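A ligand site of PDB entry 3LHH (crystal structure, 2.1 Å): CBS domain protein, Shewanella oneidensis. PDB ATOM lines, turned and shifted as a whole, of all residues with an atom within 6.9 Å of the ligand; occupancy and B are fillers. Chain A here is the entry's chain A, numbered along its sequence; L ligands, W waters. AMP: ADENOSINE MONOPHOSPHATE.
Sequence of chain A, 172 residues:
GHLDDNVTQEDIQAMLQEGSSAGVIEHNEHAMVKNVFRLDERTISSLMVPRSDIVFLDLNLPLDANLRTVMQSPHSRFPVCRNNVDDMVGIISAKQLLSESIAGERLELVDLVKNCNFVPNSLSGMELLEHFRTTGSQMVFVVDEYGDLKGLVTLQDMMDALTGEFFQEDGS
OD2 of Asp 157 is in hydrogen-bond range of O2' of the ligand (2.5 Å).
The side-chain hydroxyl (OG1) of Thr 154 lies within hydrogen-bond range of an oxygen (O3') of the ligand, at 2.7 Å.
The backbone NH of Ser 76 lies within hydrogen-bond range of an oxygen (O2P) of the ligand.
The side-chain hydroxyl (OG) of Ser 76 lies within hydrogen-bond range of an oxygen (O2P) of the ligand.
O1P of the ligand is in hydrogen-bond range of ND1 of His 75 (2.9 Å).
N of Val 55 sits at hydrogen-bond distance from N1 of the ligand, at 3.0 Å.
O of Val 55 is in hydrogen-bond range of N6 of the ligand (3.1 Å).
O of Arg 77 lies within hydrogen-bond range of N6 of the ligand, at 3.1 Å.
The backbone NH (N) of Asp 157 is in hydrogen-bond range of the side-chain hydroxyl (OG1) of Thr 154 (3.0 Å).
N of His 75 sits close to OG of Ser 73, at 3.2 Å.
N of Val 49 sits at hydrogen-bond distance from O of Leu 152 (2.7 Å).
Val 49 touches the ligand (CG2 to O2', 3.7 Å).
Asp 53 touches the ligand (O to C2, 3.3 Å).
Ile 54 touches the ligand (CA to C2, 3.9 Å).
Pro 79 touches the ligand.
Met 139 touches the ligand.
CB of Gln 156 touches O3' of the ligand, 3.6 Å away.
Hydrophobic or aromatic side chains that line the ligand: Val 49, Val 55, His 75, Pro 79 and Met 139.
Of the 24 residues printed, 12 come within 4 Å of the ligand.
Water W2 lies within hydrogen-bond range of the backbone NH of Arg 77, an oxygen (O2P) of the ligand and the backbone NH of Ser 76.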
ATOM      1  N   LEU A  47     -15.369 -23.639 -33.801  1.00  0.00           N
ATOM      2  CA  LEU A  47     -15.708 -22.757 -32.675  1.00  0.00           C
ATOM      3  C   LEU A  47     -14.784 -21.546 -32.686  1.00  0.00           C
ATOM      4  O   LEU A  47     -14.951 -20.590 -31.940  1.00  0.00           O
ATOM      5  CB  LEU A  47     -15.579 -23.501 -31.342  1.00  0.00           C
ATOM      6  CG  LEU A  47     -16.123 -24.933 -31.328  1.00  0.00           C
ATOM      7  CD1 LEU A  47     -15.231 -25.871 -32.127  1.00  0.00           C
ATOM      8  CD2 LEU A  47     -16.256 -25.436 -29.913  1.00  0.00           C
ATOM      9  N   MET A  48     -13.793 -21.629 -33.562  1.00  0.00           N
ATOM     10  CA  MET A  48     -12.736 -20.642 -33.640  1.00  0.00           C
ATOM     11  C   MET A  48     -13.193 -19.329 -34.257  1.00  0.00           C
ATOM     12  O   MET A  48     -13.987 -19.317 -35.196  1.00  0.00           O
ATOM     13  CB  MET A  48     -11.643 -21.226 -34.515  1.00  0.00           C
ATOM     14  CG  MET A  48     -10.353 -20.480 -34.498  1.00  0.00           C
ATOM     15  SD  MET A  48      -8.997 -21.695 -35.144  1.00  0.00           S
ATOM     16  CE  MET A  48      -9.590 -21.914 -36.986  1.00  0.00           C
ATOM     17  N   VAL A  49     -12.678 -18.219 -33.725  1.00  0.00           N
ATOM     18  CA  VAL A  49     -12.692 -16.962 -34.464  1.00  0.00           C
ATOM     19  C   VAL A  49     -11.464 -16.972 -35.392  1.00  0.00           C
ATOM     20  O   VAL A  49     -10.345 -16.906 -34.914  1.00  0.00           O
ATOM     21  CB  VAL A  49     -12.613 -15.740 -33.540  1.00  0.00           C
ATOM     22  CG1 VAL A  49     -12.432 -14.452 -34.354  1.00  0.00           C
ATOM     23  CG2 VAL A  49     -13.839 -15.651 -32.611  1.00  0.00           C
ATOM     24  N   PRO A  50     -11.683 -17.061 -36.722  1.00  0.00           N
ATOM     25  CA  PRO A  50     -10.588 -17.145 -37.702  1.00  0.00           C
ATOM     26  C   PRO A  50      -9.672 -15.929 -37.603  1.00  0.00           C
ATOM     27  O   PRO A  50     -10.150 -14.836 -37.294  1.00  0.00           O
ATOM     28  CB  PRO A  50     -11.314 -17.096 -39.051  1.00  0.00           C
ATOM     29  CG  PRO A  50     -12.774 -17.304 -38.745  1.00  0.00           C
ATOM     30  CD  PRO A  50     -12.977 -16.786 -37.369  1.00  0.00           C
ATOM     31  N   ASP A  53     -10.901 -12.617 -38.862  1.00  0.00           N
ATOM     32  CA  ASP A  53     -11.966 -11.941 -38.111  1.00  0.00           C
ATOM     33  C   ASP A  53     -11.471 -11.349 -36.789  1.00  0.00           C
ATOM     34  O   ASP A  53     -12.248 -10.725 -36.085  1.00  0.00           O
ATOM     35  CB  ASP A  53     -13.133 -12.908 -37.819  1.00  0.00           C
ATOM     36  CG  ASP A  53     -13.889 -13.339 -39.077  1.00  0.00           C
ATOM     37  OD1 ASP A  53     -13.515 -12.918 -40.196  1.00  0.00           O
ATOM     38  OD2 ASP A  53     -14.872 -14.103 -38.953  1.00  0.00           O
ATOM     39  N   ILE A  54     -10.198 -11.567 -36.447  1.00  0.00           N
ATOM     40  CA  ILE A  54      -9.668 -11.051 -35.185  1.00  0.00           C
ATOM     41  C   ILE A  54      -9.478  -9.539 -35.194  1.00  0.00           C
ATOM     42  O   ILE A  54      -8.801  -9.010 -36.072  1.00  0.00           O
ATOM     43  CB  ILE A  54      -8.314 -11.681 -34.803  1.00  0.00           C
ATOM     44  CG1 ILE A  54      -8.473 -13.186 -34.512  1.00  0.00           C
ATOM     45  CG2 ILE A  54      -7.738 -10.978 -33.598  1.00  0.00           C
ATOM     46  CD1 ILE A  54      -7.181 -13.857 -34.061  1.00  0.00           C
ATOM     47  N   VAL A  55     -10.039  -8.856 -34.201  1.00  0.00           N
ATOM     48  CA  VAL A  55      -9.849  -7.413 -34.065  1.00  0.00           C
ATOM     49  C   VAL A  55      -8.762  -7.194 -33.043  1.00  0.00           C
ATOM     50  O   VAL A  55      -8.895  -7.660 -31.912  1.00  0.00           O
ATOM     51  CB  VAL A  55     -11.155  -6.735 -33.581  1.00  0.00           C
ATOM     52  CG1 VAL A  55     -10.915  -5.254 -33.345  1.00  0.00           C
ATOM     53  CG2 VAL A  55     -12.281  -6.954 -34.591  1.00  0.00           C
ATOM     54  N   PHE A  56      -7.695  -6.495 -33.413  1.00  0.00           N
ATOM     55  CA  PHE A  56      -6.492  -6.471 -32.582  1.00  0.00           C
ATOM     56  C   PHE A  56      -5.866  -5.087 -32.452  1.00  0.00           C
ATOM     57  O   PHE A  56      -6.133  -4.198 -33.266  1.00  0.00           O
ATOM     58  CB  PHE A  56      -5.441  -7.461 -33.118  1.00  0.00           C
ATOM     59  CG  PHE A  56      -4.901  -7.099 -34.486  1.00  0.00           C
ATOM     60  CD1 PHE A  56      -5.480  -7.602 -35.630  1.00  0.00           C
ATOM     61  CD2 PHE A  56      -3.790  -6.272 -34.605  1.00  0.00           C
ATOM     62  CE1 PHE A  56      -4.978  -7.280 -36.887  1.00  0.00           C
ATOM     63  CE2 PHE A  56      -3.285  -5.936 -35.861  1.00  0.00           C
ATOM     64  CZ  PHE A  56      -3.884  -6.450 -36.997  1.00  0.00           C
ATOM     65  N   SER A  73     -15.504  -0.917 -31.758  1.00  0.00           N
ATOM     66  CA  SER A  73     -15.784  -2.333 -31.544  1.00  0.00           C
ATOM     67  C   SER A  73     -16.516  -2.543 -30.215  1.00  0.00           C
ATOM     68  O   SER A  73     -16.302  -1.771 -29.269  1.00  0.00           O
ATOM     69  CB  SER A  73     -14.463  -3.116 -31.551  1.00  0.00           C
ATOM     70  OG  SER A  73     -14.682  -4.449 -31.149  1.00  0.00           O
ATOM     71  N   PRO A  74     -17.386  -3.564 -30.144  1.00  0.00           N
ATOM     72  CA  PRO A  74     -18.048  -3.929 -28.873  1.00  0.00           C
ATOM     73  C   PRO A  74     -17.189  -4.837 -27.965  1.00  0.00           C
ATOM     74  O   PRO A  74     -17.523  -4.986 -26.791  1.00  0.00           O
ATOM     75  CB  PRO A  74     -19.281  -4.722 -29.337  1.00  0.00           C
ATOM     76  CG  PRO A  74     -19.035  -5.072 -30.811  1.00  0.00           C
ATOM     77  CD  PRO A  74     -17.672  -4.542 -31.200  1.00  0.00           C
ATOM     78  N   HIS A  75     -16.125  -5.441 -28.489  1.00  0.00           N
ATOM     79  CA  HIS A  75     -15.375  -6.461 -27.723  1.00  0.00           C
ATOM     80  C   HIS A  75     -14.776  -6.010 -26.402  1.00  0.00           C
ATOM     81  O   HIS A  75     -14.263  -4.914 -26.306  1.00  0.00           O
ATOM     82  CB  HIS A  75     -14.289  -7.094 -28.576  1.00  0.00           C
ATOM     83  CG  HIS A  75     -14.797  -7.664 -29.864  1.00  0.00           C
ATOM     84  ND1 HIS A  75     -15.918  -8.469 -29.914  1.00  0.00           N
ATOM     85  CD2 HIS A  75     -14.366  -7.522 -31.131  1.00  0.00           C
ATOM     86  CE1 HIS A  75     -16.139  -8.812 -31.171  1.00  0.00           C
ATOM     87  NE2 HIS A  75     -15.208  -8.254 -31.931  1.00  0.00           N
ATOM     88  N   SER A  76     -14.822  -6.876 -25.387  1.00  0.00           N
ATOM     89  CA  SER A  76     -14.253  -6.549 -24.082  1.00  0.00           C
ATOM     90  C   SER A  76     -12.744  -6.693 -24.025  1.00  0.00           C
ATOM     91  O   SER A  76     -12.073  -6.030 -23.222  1.00  0.00           O
ATOM     92  CB  SER A  76     -14.866  -7.443 -22.979  1.00  0.00           C
ATOM     93  OG  SER A  76     -16.265  -7.300 -22.942  1.00  0.00           O
ATOM     94  N   ARG A  77     -12.196  -7.596 -24.829  1.00  0.00           N
ATOM     95  CA  ARG A  77     -10.755  -7.856 -24.798  1.00  0.00           C
ATOM     96  C   ARG A  77     -10.164  -7.884 -26.205  1.00  0.00           C
ATOM     97  O   ARG A  77     -10.797  -8.348 -27.146  1.00  0.00           O
ATOM     98  CB  ARG A  77     -10.450  -9.167 -24.060  1.00  0.00           C
ATOM     99  CG  ARG A  77     -11.198  -9.330 -22.732  1.00  0.00           C
ATOM    100  CD  ARG A  77     -10.598 -10.420 -21.840  1.00  0.00           C
ATOM    101  NE  ARG A  77      -9.490  -9.903 -21.039  1.00  0.00           N
ATOM    102  CZ  ARG A  77      -9.642  -9.096 -19.990  1.00  0.00           C
ATOM    103  NH1 ARG A  77     -10.846  -8.705 -19.613  1.00  0.00           N
ATOM    104  NH2 ARG A  77      -8.575  -8.667 -19.340  1.00  0.00           N
ATOM    105  N   PHE A  78      -8.933  -7.388 -26.343  1.00  0.00           N
ATOM    106  CA  PHE A  78      -8.269  -7.339 -27.641  1.00  0.00           C
ATOM    107  C   PHE A  78      -6.890  -7.948 -27.574  1.00  0.00           C
ATOM    108  O   PHE A  78      -6.085  -7.549 -26.741  1.00  0.00           O
ATOM    109  CB  PHE A  78      -8.144  -5.886 -28.105  1.00  0.00           C
ATOM    110  CG  PHE A  78      -9.473  -5.230 -28.345  1.00  0.00           C
ATOM    111  CD1 PHE A  78     -10.026  -5.230 -29.615  1.00  0.00           C
ATOM    112  CD2 PHE A  78     -10.178  -4.622 -27.319  1.00  0.00           C
ATOM    113  CE1 PHE A  78     -11.259  -4.606 -29.861  1.00  0.00           C
ATOM    114  CE2 PHE A  78     -11.420  -4.018 -27.554  1.00  0.00           C
ATOM    115  CZ  PHE A  78     -11.951  -4.015 -28.828  1.00  0.00           C
ATOM    116  N   PRO A  79      -6.602  -8.915 -28.474  1.00  0.00           N
ATOM    117  CA  PRO A  79      -5.237  -9.369 -28.687  1.00  0.00           C
ATOM    118  C   PRO A  79      -4.388  -8.189 -29.097  1.00  0.00           C
ATOM    119  O   PRO A  79      -4.864  -7.301 -29.808  1.00  0.00           O
ATOM    120  CB  PRO A  79      -5.370 -10.349 -29.865  1.00  0.00           C
ATOM    121  CG  PRO A  79      -6.891 -10.685 -29.923  1.00  0.00           C
ATOM    122  CD  PRO A  79      -7.543  -9.450 -29.471  1.00  0.00           C
ATOM    123  N   MET A 139      -9.736 -15.953 -23.206  1.00  0.00           N
ATOM    124  CA  MET A 139      -9.334 -16.025 -24.607  1.00  0.00           C
ATOM    125  C   MET A 139      -8.048 -16.847 -24.769  1.00  0.00           C
ATOM    126  O   MET A 139      -7.103 -16.665 -24.014  1.00  0.00           O
ATOM    127  CB  MET A 139      -9.125 -14.595 -25.079  1.00  0.00           C
ATOM    128  CG  MET A 139      -8.645 -14.393 -26.485  1.00  0.00           C
ATOM    129  SD  MET A 139      -8.704 -12.462 -26.902  1.00  0.00           S
ATOM    130  CE  MET A 139     -10.633 -12.197 -26.962  1.00  0.00           C
ATOM    131  N   LEU A 152      -8.598 -17.623 -32.752  1.00  0.00           N
ATOM    132  CA  LEU A 152      -8.708 -17.607 -31.305  1.00  0.00           C
ATOM    133  C   LEU A 152     -10.007 -18.230 -30.857  1.00  0.00           C
ATOM    134  O   LEU A 152     -10.986 -18.276 -31.609  1.00  0.00           O
ATOM    135  CB  LEU A 152      -8.572 -16.182 -30.739  1.00  0.00           C
ATOM    136  CG  LEU A 152      -9.607 -15.124 -31.091  1.00  0.00           C
ATOM    137  CD1 LEU A 152     -10.880 -15.267 -30.280  1.00  0.00           C
ATOM    138  CD2 LEU A 152      -8.980 -13.758 -30.851  1.00  0.00           C
ATOM    139  N   VAL A 153     -10.000 -18.760 -29.640  1.00  0.00           N
ATOM    140  CA  VAL A 153     -11.217 -19.275 -29.013  1.00  0.00           C
ATOM    141  C   VAL A 153     -11.499 -18.523 -27.724  1.00  0.00           C
ATOM    142  O   VAL A 153     -10.586 -18.235 -26.955  1.00  0.00           O
ATOM    143  CB  VAL A 153     -11.093 -20.789 -28.728  1.00  0.00           C
ATOM    144  CG1 VAL A 153     -12.430 -21.350 -28.220  1.00  0.00           C
ATOM    145  CG2 VAL A 153     -10.707 -21.489 -29.968  1.00  0.00           C
ATOM    146  N   THR A 154     -12.772 -18.187 -27.496  1.00  0.00           N
ATOM    147  CA  THR A 154     -13.161 -17.574 -26.234  1.00  0.00           C
ATOM    148  C   THR A 154     -13.925 -18.548 -25.318  1.00  0.00           C
ATOM    149  O   THR A 154     -14.598 -19.474 -25.774  1.00  0.00           O
ATOM    150  CB  THR A 154     -14.040 -16.318 -26.448  1.00  0.00           C
ATOM    151  OG1 THR A 154     -15.314 -16.699 -26.966  1.00  0.00           O
ATOM    152  CG2 THR A 154     -13.359 -15.348 -27.409  1.00  0.00           C
ATOM    153  N   LEU A 155     -13.827 -18.321 -24.018  1.00  0.00           N
ATOM    154  CA  LEU A 155     -14.595 -19.110 -23.060  1.00  0.00           C
ATOM    155  C   LEU A 155     -16.078 -18.982 -23.400  1.00  0.00           C
ATOM    156  O   LEU A 155     -16.814 -19.982 -23.446  1.00  0.00           O
ATOM    157  CB  LEU A 155     -14.320 -18.609 -21.650  1.00  0.00           C
ATOM    158  CG  LEU A 155     -15.181 -19.262 -20.568  1.00  0.00           C
ATOM    159  CD1 LEU A 155     -14.797 -20.698 -20.420  1.00  0.00           C
ATOM    160  CD2 LEU A 155     -15.031 -18.505 -19.251  1.00  0.00           C
ATOM    161  N   GLN A 156     -16.493 -17.739 -23.669  1.00  0.00           N
ATOM    162  CA  GLN A 156     -17.887 -17.455 -24.020  1.00  0.00           C
ATOM    163  C   GLN A 156     -18.362 -18.367 -25.145  1.00  0.00           C
ATOM    164  O   GLN A 156     -19.422 -18.987 -25.057  1.00  0.00           O
ATOM    165  CB  GLN A 156     -18.025 -15.998 -24.458  1.00  0.00           C
ATOM    166  CG  GLN A 156     -18.921 -15.141 -23.579  1.00  0.00           C
ATOM    167  CD  GLN A 156     -20.233 -14.740 -24.256  1.00  0.00           C
ATOM    168  OE1 GLN A 156     -20.255 -13.894 -25.157  1.00  0.00           O
ATOM    169  NE2 GLN A 156     -21.332 -15.349 -23.824  1.00  0.00           N
ATOM    170  N   ASP A 157     -17.577 -18.441 -26.208  1.00  0.00           N
ATOM    171  CA  ASP A 157     -17.927 -19.275 -27.341  1.00  0.00           C
ATOM    172  C   ASP A 157     -17.928 -20.748 -26.960  1.00  0.00           C
ATOM    173  O   ASP A 157     -18.719 -21.535 -27.465  1.00  0.00           O
ATOM    174  CB  ASP A 157     -16.985 -19.030 -28.510  1.00  0.00           C
ATOM    175  CG  ASP A 157     -17.268 -17.710 -29.211  1.00  0.00           C
ATOM    176  OD1 ASP A 157     -18.342 -17.125 -28.927  1.00  0.00           O
ATOM    177  OD2 ASP A 157     -16.448 -17.267 -30.033  1.00  0.00           O
ATOM    178  N   MET A 158     -17.006 -21.120 -26.080  1.00  0.00           N
ATOM    179  CA  MET A 158     -16.940 -22.479 -25.592  1.00  0.00           C
ATOM    180  C   MET A 158     -18.176 -22.874 -24.785  1.00  0.00           C
ATOM    181  O   MET A 158     -18.666 -23.988 -24.896  1.00  0.00           O
ATOM    182  CB  MET A 158     -15.679 -22.681 -24.756  1.00  0.00           C
ATOM    183  CG  MET A 158     -14.458 -22.908 -25.612  1.00  0.00           C
ATOM    184  SD  MET A 158     -14.267 -24.791 -26.097  1.00  0.00           S
ATOM    185  CE  MET A 158     -16.091 -25.227 -26.652  1.00  0.00           C
ATOM    186  N   ASP A 160     -21.203 -21.300 -24.969  1.00  0.00           N
ATOM    187  CA  ASP A 160     -22.359 -21.266 -25.858  1.00  0.00           C
ATOM    188  C   ASP A 160     -22.458 -22.584 -26.598  1.00  0.00           C
ATOM    189  O   ASP A 160     -23.558 -23.085 -26.829  1.00  0.00           O
ATOM    190  CB  ASP A 160     -22.267 -20.115 -26.852  1.00  0.00           C
ATOM    191  CG  ASP A 160     -22.412 -18.764 -26.187  1.00  0.00           C
ATOM    192  OD1 ASP A 160     -22.717 -18.711 -24.979  1.00  0.00           O
ATOM    193  OD2 ASP A 160     -22.239 -17.751 -26.889  1.00  0.00           O
HETATM  194  P   AMP L   1     -17.447  -9.787 -26.476  1.00  0.00           P
HETATM  195  O1P AMP L   1     -17.714  -9.013 -27.756  1.00  0.00           O
HETATM  196  O2P AMP L   1     -16.189  -9.337 -25.780  1.00  0.00           O
HETATM  197  O3P AMP L   1     -18.639  -9.978 -25.569  1.00  0.00           O
HETATM  198  O5' AMP L   1     -17.221 -11.263 -27.063  1.00  0.00           O
HETATM  199  C5' AMP L   1     -18.307 -11.941 -27.695  1.00  0.00           C
HETATM  200  C4' AMP L   1     -17.787 -12.813 -28.851  1.00  0.00           C
HETATM  201  O4' AMP L   1     -17.168 -12.009 -29.873  1.00  0.00           O
HETATM  202  C3' AMP L   1     -16.704 -13.783 -28.417  1.00  0.00           C
HETATM  203  O3' AMP L   1     -17.227 -14.986 -27.829  1.00  0.00           O
HETATM  204  C2' AMP L   1     -15.965 -14.028 -29.721  1.00  0.00           C
HETATM  205  O2' AMP L   1     -16.817 -14.867 -30.506  1.00  0.00           O
HETATM  206  C1' AMP L   1     -15.987 -12.672 -30.378  1.00  0.00           C
HETATM  207  N9  AMP L   1     -14.810 -11.815 -30.013  1.00  0.00           N
HETATM  208  C8  AMP L   1     -14.516 -11.348 -28.786  1.00  0.00           C
HETATM  209  N7  AMP L   1     -13.407 -10.574 -28.791  1.00  0.00           N
HETATM  210  C5  AMP L   1     -12.970 -10.535 -30.058  1.00  0.00           C
HETATM  211  C6  AMP L   1     -11.852  -9.884 -30.760  1.00  0.00           C
HETATM  212  N6  AMP L   1     -10.940  -9.111 -30.096  1.00  0.00           N
HETATM  213  N1  AMP L   1     -11.764 -10.073 -32.089  1.00  0.00           N
HETATM  214  C2  AMP L   1     -12.659 -10.828 -32.768  1.00  0.00           C
HETATM  215  N3  AMP L   1     -13.700 -11.460 -32.185  1.00  0.00           N
HETATM  216  C4  AMP L   1     -13.895 -11.352 -30.858  1.00  0.00           C
HETATM  217  O   HOH W   1     -15.643 -12.190 -34.117  1.00  0.00           O
HETATM  218  O   HOH W   2     -13.423  -9.812 -26.023  1.00  0.00           O
HETATM  219  O   HOH W   3     -19.688  -8.720 -29.305  1.00  0.00           O
